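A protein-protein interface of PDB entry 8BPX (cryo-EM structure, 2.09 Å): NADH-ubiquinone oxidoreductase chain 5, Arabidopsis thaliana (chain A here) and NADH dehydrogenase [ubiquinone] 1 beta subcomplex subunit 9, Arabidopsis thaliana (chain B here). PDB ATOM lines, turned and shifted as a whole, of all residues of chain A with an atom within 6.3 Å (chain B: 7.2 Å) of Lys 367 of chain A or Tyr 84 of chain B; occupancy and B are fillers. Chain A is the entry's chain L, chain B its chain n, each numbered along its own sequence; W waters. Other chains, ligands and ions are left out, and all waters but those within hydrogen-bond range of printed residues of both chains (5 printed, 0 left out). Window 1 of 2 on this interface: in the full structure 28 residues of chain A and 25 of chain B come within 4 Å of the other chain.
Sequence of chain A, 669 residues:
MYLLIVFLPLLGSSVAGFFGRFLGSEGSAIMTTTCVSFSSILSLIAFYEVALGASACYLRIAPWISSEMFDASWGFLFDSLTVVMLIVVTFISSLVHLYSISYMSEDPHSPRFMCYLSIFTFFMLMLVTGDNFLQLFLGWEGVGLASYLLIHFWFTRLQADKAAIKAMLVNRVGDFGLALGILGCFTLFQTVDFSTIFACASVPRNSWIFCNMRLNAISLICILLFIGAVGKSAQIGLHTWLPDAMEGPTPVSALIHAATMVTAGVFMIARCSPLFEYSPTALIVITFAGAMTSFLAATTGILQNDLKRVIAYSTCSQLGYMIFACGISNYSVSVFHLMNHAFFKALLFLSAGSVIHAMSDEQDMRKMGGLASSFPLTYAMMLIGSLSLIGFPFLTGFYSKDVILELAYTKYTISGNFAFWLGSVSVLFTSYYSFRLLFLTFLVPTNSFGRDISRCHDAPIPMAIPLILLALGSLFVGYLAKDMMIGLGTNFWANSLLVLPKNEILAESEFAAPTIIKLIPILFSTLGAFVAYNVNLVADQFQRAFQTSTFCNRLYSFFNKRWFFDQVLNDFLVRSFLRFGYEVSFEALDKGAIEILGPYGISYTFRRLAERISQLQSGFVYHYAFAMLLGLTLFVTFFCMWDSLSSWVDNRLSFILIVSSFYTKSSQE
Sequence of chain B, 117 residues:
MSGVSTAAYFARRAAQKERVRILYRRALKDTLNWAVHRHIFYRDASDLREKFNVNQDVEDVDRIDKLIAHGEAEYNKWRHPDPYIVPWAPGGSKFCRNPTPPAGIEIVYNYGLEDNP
The side-chain hydroxyl (OH) of Tyr 84 of chain B lies within hydrogen-bond range of the side-chain carboxylate (OE1) of Glu 362 of chain A (2.7 Å). The guanidinium group (NH2) of Arg 366 of chain A is in salt-bridge range of the side-chain carboxylate (OD2) of Asp 82 of chain B (3.5 Å). OD1 of Asn 447 of chain A sits close to O of Val 36 of chain B (3.3 Å). The backbone NH (N) of Arg 38 of chain B lies close to the side-chain amide oxygen (OD1) of Asn 447 of chain A (3.3 Å).
OD1 of Asp 364 of chain A is in salt-bridge range of NE of Arg 366 of chain A. The backbone NH of Asn 447 of chain A is in hydrogen-bond range of the backbone carbonyl oxygen of Met 368 of chain A (2.7 Å). OD1 of Asp 30 of chain B sits at hydrogen-bond distance from ND2 of Asn 33 of chain B (3.3 Å). The backbone NH (N) of His 80 of chain B lies within hydrogen-bond range of the side-chain carboxylate (OD2) of Asp 30 of chain B (3.0 Å). A ring nitrogen (NE2) of His 80 of chain B sits close to the backbone carbonyl oxygen (O) of Asn 33 of chain B (3.4 Å). N of Asp 82 of chain B sits at hydrogen-bond distance from ND1 of His 80 of chain B (3.1 Å).
Among the printed residues, pairs that only touch across the chains: Phe 449 of chain A with Tyr 84 of chain B, Lys 367 of chain A with Leu 32 of chain B, Lys 367 of chain A with Tyr 84 of chain B, Arg 366 of chain A with Tyr 84 of chain B, Arg 366 of chain A with His 80 of chain B, Arg 366 of chain A with Pro 83 of chain B, Asp 364 of chain A with Tyr 84 of chain B, Arg 366 of chain A with Val 36 of chain B, Glu 362 of chain A with Pro 87 of chain B and Arg 366 of chain A with Asn 33 of chain B.
Lys 367 of chain A touches two residues of chain B. Lys 29 of chain B touches none of the printed residues of chain A. Asp 30 of chain B touches none of the printed residues of chain A. Of the printed residues of chain A, Asp 82 of chain B touches Arg 366. Of the printed residues of chain A, Pro 83 of chain B touches Arg 366 (3.7 Å). Of chain A, only Glu 362, Asp 364, Arg 366, Lys 367 and Phe 449 come within 4 Å of Tyr 84 of chain B. The nearest residue of chain B that does not touch Lys 367 of chain A is Arg 38 of chain B (4.5 Å). The nearest printed residue of chain A that does not touch His 80 of chain B is Asp 364 of chain A (8.3 Å).
Of the 13 printed residues of chain B, 9 touch a printed residue of chain A. Printed residues of chain B that touch a printed residue of chain A: Leu 32, Asn 33, Val 36, Arg 38, His 80, Asp 82, Pro 83, Tyr 84 and Pro 87. Printed residues of chain A that touch a printed residue of chain B: Glu 362, Asp 364, Arg 366, Lys 367, Asn 447 and Phe 449. Among the printed residues, 14 pairs touch across the chains. Among the printed residues, Asp or Glu carboxylates within 4 Å of a Lys or Arg side-chain nitrogen of the other chain: Arg 366 of chain A with Asp 82 of chain B (3.5 Å).
Water W2 bridges the backbone carbonyl oxygen (O) of Ile 85 of chain B (2.6 Å) and the side-chain carboxylate (OE2) of Glu 362 of chain A (2.7 Å). Water W4 bridges OD1 of Asn 33 of chain B and NZ of Lys 367 of chain A. Water W5 lies within hydrogen-bond range of the backbone carbonyl oxygen (O) of Val 36 of chain B (2.8 Å), the backbone carbonyl oxygen (O) of Arg 366 of chain A (2.8 Å) and the side-chain amino group (NZ) of Lys 367 of chain A (3.0 Å). Water W3 lies within hydrogen-bond range of the guanidinium group (NH1) of Arg 38 of chain B (2.8 Å), the backbone carbonyl oxygen (O) of Asn 447 of chain A (3.0 Å) and the side-chain amino group (NZ) of Lys 367 of chain A (3.0 Å). Water W1 lies within hydrogen-bond range of the side-chain carboxylate (OD2) of Asp 364 of chain A (2.9 Å) and the backbone NH (N) of Ile 85 of chain B (3.1 Å).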
ATOM      1  N   MET A 359      22.910  26.735  -9.236  1.00  0.00           N
ATOM      2  CA  MET A 359      21.970  25.928  -9.999  1.00  0.00           C
ATOM      3  C   MET A 359      22.531  25.508 -11.354  1.00  0.00           C
ATOM      4  O   MET A 359      21.767  25.282 -12.296  1.00  0.00           O
ATOM      5  CB  MET A 359      20.660  26.689 -10.177  1.00  0.00           C
ATOM      6  CG  MET A 359      19.818  26.796  -8.921  1.00  0.00           C
ATOM      7  SD  MET A 359      19.766  25.270  -7.976  1.00  0.00           S
ATOM      8  CE  MET A 359      18.330  24.500  -8.718  1.00  0.00           C
ATOM      9  N   GLU A 362      21.481  27.583 -14.430  1.00  0.00           N
ATOM     10  CA  GLU A 362      20.074  27.736 -14.767  1.00  0.00           C
ATOM     11  C   GLU A 362      19.635  29.150 -14.412  1.00  0.00           C
ATOM     12  O   GLU A 362      19.887  29.628 -13.302  1.00  0.00           O
ATOM     13  CB  GLU A 362      19.221  26.702 -14.029  1.00  0.00           C
ATOM     14  CG  GLU A 362      17.735  26.799 -14.322  1.00  0.00           C
ATOM     15  CD  GLU A 362      17.409  26.546 -15.785  1.00  0.00           C
ATOM     16  OE1 GLU A 362      17.635  25.415 -16.264  1.00  0.00           O
ATOM     17  OE2 GLU A 362      16.930  27.478 -16.458  1.00  0.00           O
ATOM     18  N   ASP A 364      16.320  30.295 -15.680  1.00  0.00           N
ATOM     19  CA  ASP A 364      14.877  30.359 -15.853  1.00  0.00           C
ATOM     20  C   ASP A 364      14.190  30.073 -14.524  1.00  0.00           C
ATOM     21  O   ASP A 364      14.398  29.011 -13.929  1.00  0.00           O
ATOM     22  CB  ASP A 364      14.423  29.369 -16.924  1.00  0.00           C
ATOM     23  CG  ASP A 364      13.188  29.834 -17.657  1.00  0.00           C
ATOM     24  OD1 ASP A 364      12.079  29.663 -17.116  1.00  0.00           O
ATOM     25  OD2 ASP A 364      13.321  30.368 -18.773  1.00  0.00           O
ATOM     26  N   MET A 365      13.363  31.016 -14.071  1.00  0.00           N
ATOM     27  CA  MET A 365      12.676  30.866 -12.794  1.00  0.00           C
ATOM     28  C   MET A 365      11.651  29.740 -12.816  1.00  0.00           C
ATOM     29  O   MET A 365      11.284  29.239 -11.751  1.00  0.00           O
ATOM     30  CB  MET A 365      12.006  32.184 -12.397  1.00  0.00           C
ATOM     31  CG  MET A 365      12.989  33.274 -12.009  1.00  0.00           C
ATOM     32  SD  MET A 365      12.227  34.828 -11.503  1.00  0.00           S
ATOM     33  CE  MET A 365      11.264  35.250 -12.950  1.00  0.00           C
ATOM     34  N   ARG A 366      11.189  29.330 -13.997  1.00  0.00           N
ATOM     35  CA  ARG A 366      10.253  28.219 -14.093  1.00  0.00           C
ATOM     36  C   ARG A 366      10.893  26.874 -13.775  1.00  0.00           C
ATOM     37  O   ARG A 366      10.169  25.885 -13.641  1.00  0.00           O
ATOM     38  CB  ARG A 366       9.627  28.170 -15.488  1.00  0.00           C
ATOM     39  CG  ARG A 366       9.021  29.473 -15.974  1.00  0.00           C
ATOM     40  CD  ARG A 366       8.569  29.310 -17.410  1.00  0.00           C
ATOM     41  NE  ARG A 366       9.674  29.502 -18.342  1.00  0.00           N
ATOM     42  CZ  ARG A 366       9.559  30.037 -19.548  1.00  0.00           C
ATOM     43  NH1 ARG A 366       8.382  30.361 -20.051  1.00  0.00           N
ATOM     44  NH2 ARG A 366      10.654  30.235 -20.275  1.00  0.00           N
ATOM     45  N   LYS A 367      12.181  26.793 -13.591  1.00  0.00           N
ATOM     46  CA  LYS A 367      12.910  25.533 -13.304  1.00  0.00           C
ATOM     47  C   LYS A 367      13.638  25.719 -11.974  1.00  0.00           C
ATOM     48  O   LYS A 367      14.694  25.197 -11.821  1.00  0.00           O
ATOM     49  CB  LYS A 367      13.776  25.115 -14.528  1.00  0.00           C
ATOM     50  CG  LYS A 367      13.049  24.912 -15.840  1.00  0.00           C
ATOM     51  CD  LYS A 367      12.162  23.713 -15.859  1.00  0.00           C
ATOM     52  CE  LYS A 367      11.262  23.717 -17.072  1.00  0.00           C
ATOM     53  NZ  LYS A 367      10.097  22.832 -16.891  1.00  0.00           N
ATOM     54  N   MET A 368      13.028  26.419 -11.044  1.00  0.00           N
ATOM     55  CA  MET A 368      13.625  26.745  -9.757  1.00  0.00           C
ATOM     56  C   MET A 368      12.569  26.444  -8.698  1.00  0.00           C
ATOM     57  O   MET A 368      11.625  25.684  -8.934  1.00  0.00           O
ATOM     58  CB  MET A 368      14.113  28.203  -9.742  1.00  0.00           C
ATOM     59  CG  MET A 368      15.523  28.403 -10.284  1.00  0.00           C
ATOM     60  SD  MET A 368      15.948  30.143 -10.507  1.00  0.00           S
ATOM     61  CE  MET A 368      16.882  30.094 -12.039  1.00  0.00           C
ATOM     62  N   GLY A 369      12.732  27.009  -7.516  1.00  0.00           N
ATOM     63  CA  GLY A 369      11.703  26.865  -6.507  1.00  0.00           C
ATOM     64  C   GLY A 369      12.111  25.904  -5.412  1.00  0.00           C
ATOM     65  O   GLY A 369      12.921  24.996  -5.614  1.00  0.00           O
ATOM     66  N   THR A 446       9.191  22.906  -5.674  1.00  0.00           N
ATOM     67  CA  THR A 446      10.277  23.016  -6.639  1.00  0.00           C
ATOM     68  C   THR A 446       9.855  22.546  -8.028  1.00  0.00           C
ATOM     69  O   THR A 446       9.187  21.520  -8.190  1.00  0.00           O
ATOM     70  CB  THR A 446      11.502  22.226  -6.161  1.00  0.00           C
ATOM     71  OG1 THR A 446      12.575  22.396  -7.096  1.00  0.00           O
ATOM     72  CG2 THR A 446      11.193  20.746  -6.023  1.00  0.00           C
ATOM     73  N   ASN A 447      10.242  23.325  -9.034  1.00  0.00           N
ATOM     74  CA  ASN A 447      10.026  22.994 -10.434  1.00  0.00           C
ATOM     75  C   ASN A 447      11.339  22.695 -11.143  1.00  0.00           C
ATOM     76  O   ASN A 447      11.402  22.727 -12.375  1.00  0.00           O
ATOM     77  CB  ASN A 447       9.296  24.133 -11.144  1.00  0.00           C
ATOM     78  CG  ASN A 447       7.847  24.240 -10.740  1.00  0.00           C
ATOM     79  OD1 ASN A 447       7.123  23.248 -10.698  1.00  0.00           O
ATOM     80  ND2 ASN A 447       7.411  25.457 -10.447  1.00  0.00           N
ATOM     81  N   SER A 448      12.393  22.421 -10.385  1.00  0.00           N
ATOM     82  CA  SER A 448      13.726  22.274 -10.939  1.00  0.00           C
ATOM     83  C   SER A 448      13.996  20.830 -11.354  1.00  0.00           C
ATOM     84  O   SER A 448      13.187  19.925 -11.152  1.00  0.00           O
ATOM     85  CB  SER A 448      14.775  22.738  -9.931  1.00  0.00           C
ATOM     86  OG  SER A 448      14.796  21.898  -8.799  1.00  0.00           O
ATOM     87  N   PHE A 449      15.191  20.609 -11.858  1.00  0.00           N
ATOM     88  CA  PHE A 449      15.662  19.289 -12.291  1.00  0.00           C
ATOM     89  C   PHE A 449      16.389  18.674 -11.088  1.00  0.00           C
ATOM     90  O   PHE A 449      17.064  19.411 -10.387  1.00  0.00           O
ATOM     91  CB  PHE A 449      16.551  19.530 -13.525  1.00  0.00           C
ATOM     92  CG  PHE A 449      15.850  19.935 -14.796  1.00  0.00           C
ATOM     93  CD1 PHE A 449      15.750  21.265 -15.164  1.00  0.00           C
ATOM     94  CD2 PHE A 449      15.340  18.984 -15.664  1.00  0.00           C
ATOM     95  CE1 PHE A 449      15.134  21.641 -16.347  1.00  0.00           C
ATOM     96  CE2 PHE A 449      14.720  19.357 -16.846  1.00  0.00           C
ATOM     97  CZ  PHE A 449      14.619  20.684 -17.189  1.00  0.00           C
ATOM     98  N   ASP A 452      20.117  19.296 -10.849  1.00  0.00           N
ATOM     99  CA  ASP A 452      20.530  20.637 -10.365  1.00  0.00           C
ATOM    100  C   ASP A 452      20.545  20.676  -8.821  1.00  0.00           C
ATOM    101  O   ASP A 452      21.530  21.083  -8.301  1.00  0.00           O
ATOM    102  CB  ASP A 452      19.718  21.754 -11.052  1.00  0.00           C
ATOM    103  CG  ASP A 452      19.984  21.930 -12.530  1.00  0.00           C
ATOM    104  OD1 ASP A 452      21.151  21.851 -12.937  1.00  0.00           O
ATOM    105  OD2 ASP A 452      19.024  22.155 -13.251  1.00  0.00           O
ATOM    106  N   LYS B  29       5.542  19.901 -24.509  1.00  0.00           N
ATOM    107  CA  LYS B  29       6.653  20.692 -23.938  1.00  0.00           C
ATOM    108  C   LYS B  29       6.186  22.134 -23.707  1.00  0.00           C
ATOM    109  O   LYS B  29       6.514  22.691 -22.667  1.00  0.00           O
ATOM    110  CB  LYS B  29       7.931  20.413 -24.746  1.00  0.00           C
ATOM    111  CG  LYS B  29       8.811  19.368 -24.074  1.00  0.00           C
ATOM    112  CD  LYS B  29      10.187  19.198 -24.647  1.00  0.00           C
ATOM    113  CE  LYS B  29      10.174  18.286 -25.848  1.00  0.00           C
ATOM    114  NZ  LYS B  29       9.230  17.161 -25.650  1.00  0.00           N
ATOM    115  N   ASP B  30       5.320  22.615 -24.582  1.00  0.00           N
ATOM    116  CA  ASP B  30       4.764  23.958 -24.469  1.00  0.00           C
ATOM    117  C   ASP B  30       3.707  24.036 -23.361  1.00  0.00           C
ATOM    118  O   ASP B  30       3.551  25.093 -22.845  1.00  0.00           O
ATOM    119  CB  ASP B  30       4.243  24.412 -25.820  1.00  0.00           C
ATOM    120  CG  ASP B  30       4.335  25.905 -26.014  1.00  0.00           C
ATOM    121  OD1 ASP B  30       5.462  26.408 -26.076  1.00  0.00           O
ATOM    122  OD2 ASP B  30       3.274  26.541 -26.089  1.00  0.00           O
ATOM    123  N   LEU B  32       3.980  22.723 -20.566  1.00  0.00           N
ATOM    124  CA  LEU B  32       4.823  22.997 -19.392  1.00  0.00           C
ATOM    125  C   LEU B  32       5.269  24.461 -19.341  1.00  0.00           C
ATOM    126  O   LEU B  32       5.273  24.968 -18.240  1.00  0.00           O
ATOM    127  CB  LEU B  32       5.938  21.957 -19.316  1.00  0.00           C
ATOM    128  CG  LEU B  32       6.824  21.966 -18.072  1.00  0.00           C
ATOM    129  CD1 LEU B  32       6.008  21.861 -16.798  1.00  0.00           C
ATOM    130  CD2 LEU B  32       7.825  20.835 -18.149  1.00  0.00           C
ATOM    131  N   ASN B  33       5.569  25.111 -20.461  1.00  0.00           N
ATOM    132  CA  ASN B  33       5.905  26.555 -20.506  1.00  0.00           C
ATOM    133  C   ASN B  33       4.761  27.435 -19.995  1.00  0.00           C
ATOM    134  O   ASN B  33       5.045  28.416 -19.359  1.00  0.00           O
ATOM    135  CB  ASN B  33       6.387  27.004 -21.902  1.00  0.00           C
ATOM    136  CG  ASN B  33       7.617  26.288 -22.405  1.00  0.00           C
ATOM    137  OD1 ASN B  33       8.576  26.138 -21.674  1.00  0.00           O
ATOM    138  ND2 ASN B  33       7.605  25.873 -23.659  1.00  0.00           N
ATOM    139  N   VAL B  36       4.034  26.068 -15.750  1.00  0.00           N
ATOM    140  CA  VAL B  36       5.129  26.314 -14.772  1.00  0.00           C
ATOM    141  C   VAL B  36       5.039  25.308 -13.621  1.00  0.00           C
ATOM    142  O   VAL B  36       5.953  24.558 -13.510  1.00  0.00           O
ATOM    143  CB  VAL B  36       5.271  27.816 -14.355  1.00  0.00           C
ATOM    144  CG1 VAL B  36       6.400  28.045 -13.371  1.00  0.00           C
ATOM    145  CG2 VAL B  36       5.353  28.736 -15.556  1.00  0.00           C
ATOM    146  N   ARG B  38       4.171  22.019 -11.633  1.00  0.00           N
ATOM    147  CA  ARG B  38       3.932  20.573 -11.928  1.00  0.00           C
ATOM    148  C   ARG B  38       2.452  20.167 -11.871  1.00  0.00           C
ATOM    149  O   ARG B  38       1.961  19.693 -12.871  1.00  0.00           O
ATOM    150  CB  ARG B  38       4.798  19.730 -10.986  1.00  0.00           C
ATOM    151  CG  ARG B  38       6.285  20.055 -10.989  1.00  0.00           C
ATOM    152  CD  ARG B  38       7.002  20.046 -12.327  1.00  0.00           C
ATOM    153  NE  ARG B  38       7.060  18.721 -12.904  1.00  0.00           N
ATOM    154  CZ  ARG B  38       7.651  18.397 -14.049  1.00  0.00           C
ATOM    155  NH1 ARG B  38       8.254  19.312 -14.781  1.00  0.00           N
ATOM    156  NH2 ARG B  38       7.632  17.141 -14.452  1.00  0.00           N
ATOM    157  N   HIS B  80       4.035  29.299 -26.858  1.00  0.00           N
ATOM    158  CA  HIS B  80       4.533  30.216 -25.831  1.00  0.00           C
ATOM    159  C   HIS B  80       5.618  31.124 -26.398  1.00  0.00           C
ATOM    160  O   HIS B  80       6.584  30.633 -26.989  1.00  0.00           O
ATOM    161  CB  HIS B  80       5.065  29.451 -24.625  1.00  0.00           C
ATOM    162  CG  HIS B  80       5.132  30.267 -23.371  1.00  0.00           C
ATOM    163  ND1 HIS B  80       5.910  31.401 -23.264  1.00  0.00           N
ATOM    164  CD2 HIS B  80       4.497  30.134 -22.182  1.00  0.00           C
ATOM    165  CE1 HIS B  80       5.764  31.919 -22.058  1.00  0.00           C
ATOM    166  NE2 HIS B  80       4.912  31.170 -21.382  1.00  0.00           N
ATOM    167  N   ASP B  82       8.109  32.688 -25.113  1.00  0.00           N
ATOM    168  CA  ASP B  82       9.441  32.567 -24.522  1.00  0.00           C
ATOM    169  C   ASP B  82       9.608  31.159 -23.962  1.00  0.00           C
ATOM    170  O   ASP B  82       9.557  30.949 -22.744  1.00  0.00           O
ATOM    171  CB  ASP B  82       9.655  33.647 -23.457  1.00  0.00           C
ATOM    172  CG  ASP B  82      10.954  33.483 -22.706  1.00  0.00           C
ATOM    173  OD1 ASP B  82      12.011  33.351 -23.356  1.00  0.00           O
ATOM    174  OD2 ASP B  82      10.917  33.480 -21.461  1.00  0.00           O
ATOM    175  N   PRO B  83       9.816  30.168 -24.828  1.00  0.00           N
ATOM    176  CA  PRO B  83       9.932  28.784 -24.352  1.00  0.00           C
ATOM    177  C   PRO B  83      11.185  28.555 -23.523  1.00  0.00           C
ATOM    178  O   PRO B  83      12.203  29.231 -23.686  1.00  0.00           O
ATOM    179  CB  PRO B  83       9.979  27.967 -25.648  1.00  0.00           C
ATOM    180  CG  PRO B  83      10.498  28.912 -26.670  1.00  0.00           C
ATOM    181  CD  PRO B  83       9.970  30.267 -26.290  1.00  0.00           C
ATOM    182  N   TYR B  84      11.098  27.577 -22.629  1.00  0.00           N
ATOM    183  CA  TYR B  84      12.256  27.173 -21.848  1.00  0.00           C
ATOM    184  C   TYR B  84      13.241  26.397 -22.713  1.00  0.00           C
ATOM    185  O   TYR B  84      12.851  25.557 -23.526  1.00  0.00           O
ATOM    186  CB  TYR B  84      11.838  26.310 -20.656  1.00  0.00           C
ATOM    187  CG  TYR B  84      13.025  25.674 -19.985  1.00  0.00           C
ATOM    188  CD1 TYR B  84      13.835  26.410 -19.130  1.00  0.00           C
ATOM    189  CD2 TYR B  84      13.375  24.355 -20.248  1.00  0.00           C
ATOM    190  CE1 TYR B  84      14.939  25.844 -18.539  1.00  0.00           C
ATOM    191  CE2 TYR B  84      14.482  23.783 -19.663  1.00  0.00           C
ATOM    192  CZ  TYR B  84      15.260  24.531 -18.808  1.00  0.00           C
ATOM    193  OH  TYR B  84      16.359  23.964 -18.218  1.00  0.00           O
ATOM    194  N   ILE B  85      14.526  26.671 -22.526  1.00  0.00           N
ATOM    195  CA  ILE B  85      15.589  25.928 -23.191  1.00  0.00           C
ATOM    196  C   ILE B  85      16.647  25.568 -22.160  1.00  0.00           C
ATOM    197  O   ILE B  85      17.042  26.411 -21.349  1.00  0.00           O
ATOM    198  CB  ILE B  85      16.218  26.719 -24.360  1.00  0.00           C
ATOM    199  CG1 ILE B  85      15.157  27.142 -25.375  1.00  0.00           C
ATOM    200  CG2 ILE B  85      17.311  25.904 -25.044  1.00  0.00           C
ATOM    201  CD1 ILE B  85      15.321  28.551 -25.880  1.00  0.00           C
ATOM    202  N   VAL B  86      17.104  24.322 -22.196  1.00  0.00           N
ATOM    203  CA  VAL B  86      18.257  23.919 -21.383  1.00  0.00           C
ATOM    204  C   VAL B  86      19.440  24.825 -21.716  1.00  0.00           C
ATOM    205  O   VAL B  86      19.698  25.090 -22.905  1.00  0.00           O
ATOM    206  CB  VAL B  86      18.599  22.439 -21.637  1.00  0.00           C
ATOM    207  CG1 VAL B  86      19.743  21.978 -20.756  1.00  0.00           C
ATOM    208  CG2 VAL B  86      17.371  21.569 -21.409  1.00  0.00           C
ATOM    209  N   PRO B  87      20.172  25.334 -20.719  1.00  0.00           N
ATOM    210  CA  PRO B  87      21.149  26.404 -20.996  1.00  0.00           C
ATOM    211  C   PRO B  87      22.217  26.054 -22.022  1.00  0.00           C
ATOM    212  O   PRO B  87      22.665  26.946 -22.750  1.00  0.00           O
ATOM    213  CB  PRO B  87      21.757  26.675 -19.613  1.00  0.00           C
ATOM    214  CG  PRO B  87      20.718  26.248 -18.656  1.00  0.00           C
ATOM    215  CD  PRO B  87      20.025  25.079 -19.276  1.00  0.00           C
HETATM  216  O   HOH W   1      15.046  28.987 -20.600  1.00  0.00           O
HETATM  217  O   HOH W   2      17.299  27.661 -19.139  1.00  0.00           O
HETATM  218  O   HOH W   3       9.247  21.863 -14.218  1.00  0.00           O
HETATM  219  O   HOH W   4       8.808  24.309 -19.684  1.00  0.00           O
HETATM  220  O   HOH W   5       8.222  24.369 -15.058  1.00  0.00           O
